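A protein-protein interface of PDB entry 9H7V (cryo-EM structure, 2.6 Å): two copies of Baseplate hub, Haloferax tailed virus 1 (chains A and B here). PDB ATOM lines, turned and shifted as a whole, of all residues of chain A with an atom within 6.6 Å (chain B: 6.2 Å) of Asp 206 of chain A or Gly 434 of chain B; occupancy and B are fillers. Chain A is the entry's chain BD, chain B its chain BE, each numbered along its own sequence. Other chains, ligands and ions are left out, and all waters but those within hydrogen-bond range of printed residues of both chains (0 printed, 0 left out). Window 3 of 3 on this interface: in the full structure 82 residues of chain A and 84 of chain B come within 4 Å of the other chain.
O of Gly 434 of chain B is in hydrogen-bond range of OG of Ser 436 of chain B, at 3.3 Å. The backbone carbonyl oxygen (O) of Thr 311 of chain A lies within hydrogen-bond range of the backbone NH (N) of Ile 205 of chain A, 2.9 Å away. The guanidinium group of Arg 487 of chain B is in hydrogen-bond range of the backbone carbonyl oxygen of Gly 434 of chain B. ND2 of Asn 439 of chain B lies within hydrogen-bond range of O of Gly 434 of chain B (2.9 Å). A ring nitrogen (ND1) of His 204 of chain A lies within hydrogen-bond range of the side-chain carboxylate of Asp 206 of chain A (3.2 Å). OD1 of Asn 439 of chain B lies within hydrogen-bond range of N of Ser 436 of chain B.
Gly 434 of chain B touches His 204 of chain A. CE1 of His 204 of chain A touches O of Leu 435 of chain B (3.9 Å). Ser 436 of chain B touches His 204 of chain A. CB of His 204 of chain A touches OG1 of Thr 438 of chain B, 3.4 Å away. Asp 206 of chain A touches Gly 434 of chain B. CG2 of Thr 438 of chain B touches OG1 of Thr 311 of chain A, 3.8 Å away.
Of the printed residues of chain B, His 204 of chain A touches Gly 434 (3.8 Å), Leu 435 (3.9 Å), Ser 436 (3.5 Å) and Thr 438 (3.4 Å). Asp 206 of chain A touches just one residue of chain B: Gly 434. Arg 207 of chain A touches none of the printed residues of chain B. Asn 432 of chain B touches none of the printed residues of chain A. Of the printed residues of chain A, Gly 434 of chain B touches His 204 and Asp 206. Of the printed residues of chain A, Leu 435 of chain B touches His 204. The nearest printed residue of chain B that does not touch His 204 of chain A is Asn 439 of chain B (5.7 Å).
Of the 9 printed residues of chain B, 4 touch a printed residue of chain A. Printed residues of chain B that touch a printed residue of chain A: Gly 434, Leu 435, Ser 436 and Thr 438. Along chain B the printed residues that touch a printed residue of chain A span positions 434 to 438. Hydrophobic or aromatic side chains of chain A within 4 Å of the printed part of chain B: His 204. Among the printed residues, 6 pairs touch across the chains. Among the printed residues, no Asp or Glu carboxylate lies within 4 Å of a Lys or Arg side-chain nitrogen of the other chain.
No position is printed for both chains.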
ATOM      1  N   HIS A 204      24.147  -0.025  -3.909  1.00  0.00           N
ATOM      2  CA  HIS A 204      24.294   1.196  -4.683  1.00  0.00           C
ATOM      3  C   HIS A 204      25.701   1.760  -4.503  1.00  0.00           C
ATOM      4  O   HIS A 204      26.204   1.840  -3.383  1.00  0.00           O
ATOM      5  CB  HIS A 204      23.198   2.202  -4.309  1.00  0.00           C
ATOM      6  CG  HIS A 204      23.334   3.524  -4.983  1.00  0.00           C
ATOM      7  ND1 HIS A 204      23.693   4.667  -4.296  1.00  0.00           N
ATOM      8  CD2 HIS A 204      23.163   3.893  -6.271  1.00  0.00           C
ATOM      9  CE1 HIS A 204      23.735   5.684  -5.132  1.00  0.00           C
ATOM     10  NE2 HIS A 204      23.414   5.235  -6.350  1.00  0.00           N
ATOM     11  N   ILE A 205      26.314   2.150  -5.628  1.00  0.00           N
ATOM     12  CA  ILE A 205      27.649   2.725  -5.654  1.00  0.00           C
ATOM     13  C   ILE A 205      27.513   4.244  -5.563  1.00  0.00           C
ATOM     14  O   ILE A 205      27.183   4.914  -6.541  1.00  0.00           O
ATOM     15  CB  ILE A 205      28.437   2.240  -6.890  1.00  0.00           C
ATOM     16  CG1 ILE A 205      28.561   0.717  -6.903  1.00  0.00           C
ATOM     17  CG2 ILE A 205      29.805   2.904  -6.965  1.00  0.00           C
ATOM     18  CD1 ILE A 205      28.355   0.124  -8.263  1.00  0.00           C
ATOM     19  N   ASP A 206      27.780   4.753  -4.355  1.00  0.00           N
ATOM     20  CA  ASP A 206      27.443   6.088  -3.882  1.00  0.00           C
ATOM     21  C   ASP A 206      28.137   7.171  -4.711  1.00  0.00           C
ATOM     22  O   ASP A 206      27.626   8.285  -4.817  1.00  0.00           O
ATOM     23  CB  ASP A 206      27.769   6.179  -2.386  1.00  0.00           C
ATOM     24  CG  ASP A 206      26.864   5.398  -1.445  1.00  0.00           C
ATOM     25  OD1 ASP A 206      25.772   4.975  -1.876  1.00  0.00           O
ATOM     26  OD2 ASP A 206      27.269   5.209  -0.279  1.00  0.00           O
ATOM     27  N   ARG A 207      29.287   6.821  -5.302  1.00  0.00           N
ATOM     28  CA  ARG A 207      30.164   7.733  -6.024  1.00  0.00           C
ATOM     29  C   ARG A 207      29.485   8.245  -7.298  1.00  0.00           C
ATOM     30  O   ARG A 207      29.526   9.443  -7.573  1.00  0.00           O
ATOM     31  CB  ARG A 207      31.499   7.029  -6.294  1.00  0.00           C
ATOM     32  CG  ARG A 207      32.636   7.925  -6.766  1.00  0.00           C
ATOM     33  CD  ARG A 207      32.597   8.121  -8.267  1.00  0.00           C
ATOM     34  NE  ARG A 207      33.861   7.925  -8.957  1.00  0.00           N
ATOM     35  CZ  ARG A 207      33.986   7.661 -10.254  1.00  0.00           C
ATOM     36  NH1 ARG A 207      35.187   7.501 -10.775  1.00  0.00           N
ATOM     37  NH2 ARG A 207      32.921   7.548 -11.028  1.00  0.00           N
ATOM     38  N   GLY A 208      28.894   7.328  -8.078  1.00  0.00           N
ATOM     39  CA  GLY A 208      28.171   7.660  -9.297  1.00  0.00           C
ATOM     40  C   GLY A 208      29.100   7.976 -10.468  1.00  0.00           C
ATOM     41  O   GLY A 208      30.317   7.885 -10.345  1.00  0.00           O
ATOM     42  N   THR A 311      23.889  -1.037  -8.497  1.00  0.00           N
ATOM     43  CA  THR A 311      23.229   0.080  -9.155  1.00  0.00           C
ATOM     44  C   THR A 311      24.111   1.322  -9.036  1.00  0.00           C
ATOM     45  O   THR A 311      24.787   1.505  -8.026  1.00  0.00           O
ATOM     46  CB  THR A 311      21.826   0.304  -8.575  1.00  0.00           C
ATOM     47  OG1 THR A 311      21.174  -0.962  -8.476  1.00  0.00           O
ATOM     48  CG2 THR A 311      20.971   1.231  -9.410  1.00  0.00           C
ATOM     49  N   ILE A 312      24.093   2.165 -10.077  1.00  0.00           N
ATOM     50  CA  ILE A 312      24.904   3.375 -10.118  1.00  0.00           C
ATOM     51  C   ILE A 312      24.159   4.486 -10.863  1.00  0.00           C
ATOM     52  O   ILE A 312      23.474   4.229 -11.851  1.00  0.00           O
ATOM     53  CB  ILE A 312      26.312   3.088 -10.695  1.00  0.00           C
ATOM     54  CG1 ILE A 312      27.273   4.265 -10.496  1.00  0.00           C
ATOM     55  CG2 ILE A 312      26.256   2.625 -12.148  1.00  0.00           C
ATOM     56  CD1 ILE A 312      28.738   3.896 -10.560  1.00  0.00           C
ATOM     57  N   ASP A 313      24.300   5.720 -10.356  1.00  0.00           N
ATOM     58  CA  ASP A 313      23.861   6.940 -11.019  1.00  0.00           C
ATOM     59  C   ASP A 313      24.813   7.251 -12.171  1.00  0.00           C
ATOM     60  O   ASP A 313      26.026   7.309 -11.966  1.00  0.00           O
ATOM     61  CB  ASP A 313      23.912   8.136 -10.062  1.00  0.00           C
ATOM     62  CG  ASP A 313      22.745   8.268  -9.096  1.00  0.00           C
ATOM     63  OD1 ASP A 313      21.617   7.883  -9.468  1.00  0.00           O
ATOM     64  OD2 ASP A 313      22.971   8.777  -7.979  1.00  0.00           O
ATOM     65  N   ASP B 431      20.794  13.260   6.325  1.00  0.00           N
ATOM     66  CA  ASP B 431      21.770  12.704   5.394  1.00  0.00           C
ATOM     67  C   ASP B 431      21.198  12.629   3.975  1.00  0.00           C
ATOM     68  O   ASP B 431      20.239  11.901   3.736  1.00  0.00           O
ATOM     69  CB  ASP B 431      22.252  11.343   5.912  1.00  0.00           C
ATOM     70  CG  ASP B 431      23.309  10.641   5.073  1.00  0.00           C
ATOM     71  OD1 ASP B 431      23.842  11.266   4.135  1.00  0.00           O
ATOM     72  OD2 ASP B 431      23.599   9.466   5.375  1.00  0.00           O
ATOM     73  N   ASN B 432      21.826  13.344   3.025  1.00  0.00           N
ATOM     74  CA  ASN B 432      21.358  13.376   1.644  1.00  0.00           C
ATOM     75  C   ASN B 432      22.141  12.417   0.742  1.00  0.00           C
ATOM     76  O   ASN B 432      21.952  12.437  -0.474  1.00  0.00           O
ATOM     77  CB  ASN B 432      21.247  14.803   1.081  1.00  0.00           C
ATOM     78  CG  ASN B 432      22.527  15.614   1.066  1.00  0.00           C
ATOM     79  OD1 ASN B 432      23.616  15.102   1.319  1.00  0.00           O
ATOM     80  ND2 ASN B 432      22.403  16.897   0.766  1.00  0.00           N
ATOM     81  N   SER B 433      22.992  11.562   1.328  1.00  0.00           N
ATOM     82  CA  SER B 433      23.856  10.688   0.543  1.00  0.00           C
ATOM     83  C   SER B 433      23.121   9.419   0.107  1.00  0.00           C
ATOM     84  O   SER B 433      22.218   8.953   0.799  1.00  0.00           O
ATOM     85  CB  SER B 433      25.133  10.359   1.280  1.00  0.00           C
ATOM     86  OG  SER B 433      24.877   9.527   2.402  1.00  0.00           O
ATOM     87  N   GLY B 434      23.524   8.890  -1.058  1.00  0.00           N
ATOM     88  CA  GLY B 434      23.225   7.532  -1.493  1.00  0.00           C
ATOM     89  C   GLY B 434      21.770   7.301  -1.894  1.00  0.00           C
ATOM     90  O   GLY B 434      21.270   6.189  -1.734  1.00  0.00           O
ATOM     91  N   LEU B 435      21.107   8.344  -2.416  1.00  0.00           N
ATOM     92  CA  LEU B 435      19.727   8.230  -2.864  1.00  0.00           C
ATOM     93  C   LEU B 435      19.653   7.298  -4.070  1.00  0.00           C
ATOM     94  O   LEU B 435      20.310   7.537  -5.084  1.00  0.00           O
ATOM     95  CB  LEU B 435      19.152   9.614  -3.185  1.00  0.00           C
ATOM     96  CG  LEU B 435      17.707   9.621  -3.685  1.00  0.00           C
ATOM     97  CD1 LEU B 435      16.746   9.101  -2.623  1.00  0.00           C
ATOM     98  CD2 LEU B 435      17.292  11.009  -4.134  1.00  0.00           C
ATOM     99  N   SER B 436      18.838   6.244  -3.935  1.00  0.00           N
ATOM    100  CA  SER B 436      18.781   5.157  -4.898  1.00  0.00           C
ATOM    101  C   SER B 436      17.474   4.380  -4.763  1.00  0.00           C
ATOM    102  O   SER B 436      16.761   4.528  -3.772  1.00  0.00           O
ATOM    103  CB  SER B 436      19.964   4.238  -4.731  1.00  0.00           C
ATOM    104  OG  SER B 436      19.995   3.682  -3.425  1.00  0.00           O
ATOM    105  N   THR B 438      17.549   1.384  -4.166  1.00  0.00           N
ATOM    106  CA  THR B 438      17.935   0.276  -3.302  1.00  0.00           C
ATOM    107  C   THR B 438      17.831   0.635  -1.817  1.00  0.00           C
ATOM    108  O   THR B 438      18.105  -0.213  -0.967  1.00  0.00           O
ATOM    109  CB  THR B 438      19.330  -0.263  -3.659  1.00  0.00           C
ATOM    110  OG1 THR B 438      20.315   0.688  -3.258  1.00  0.00           O
ATOM    111  CG2 THR B 438      19.497  -0.602  -5.124  1.00  0.00           C
ATOM    112  N   ASN B 439      17.429   1.878  -1.509  1.00  0.00           N
ATOM    113  CA  ASN B 439      17.337   2.375  -0.143  1.00  0.00           C
ATOM    114  C   ASN B 439      16.201   1.672   0.602  1.00  0.00           C
ATOM    115  O   ASN B 439      15.040   1.784   0.210  1.00  0.00           O
ATOM    116  CB  ASN B 439      17.132   3.895  -0.093  1.00  0.00           C
ATOM    117  CG  ASN B 439      18.297   4.715  -0.613  1.00  0.00           C
ATOM    118  OD1 ASN B 439      18.094   5.790  -1.171  1.00  0.00           O
ATOM    119  ND2 ASN B 439      19.515   4.233  -0.429  1.00  0.00           N
ATOM    120  N   ARG B 487      11.964   7.746  -0.615  1.00  0.00           N
ATOM    121  CA  ARG B 487      12.972   8.634  -0.063  1.00  0.00           C
ATOM    122  C   ARG B 487      13.085   9.850  -0.977  1.00  0.00           C
ATOM    123  O   ARG B 487      13.074   9.713  -2.199  1.00  0.00           O
ATOM    124  CB  ARG B 487      14.310   7.907   0.097  1.00  0.00           C
ATOM    125  CG  ARG B 487      15.315   8.636   0.977  1.00  0.00           C
ATOM    126  CD  ARG B 487      16.610   7.864   1.107  1.00  0.00           C
ATOM    127  NE  ARG B 487      17.635   8.617   1.818  1.00  0.00           N
ATOM    128  CZ  ARG B 487      18.936   8.588   1.545  1.00  0.00           C
ATOM    129  NH1 ARG B 487      19.775   9.316   2.261  1.00  0.00           N
ATOM    130  NH2 ARG B 487      19.399   7.846   0.553  1.00  0.00           N
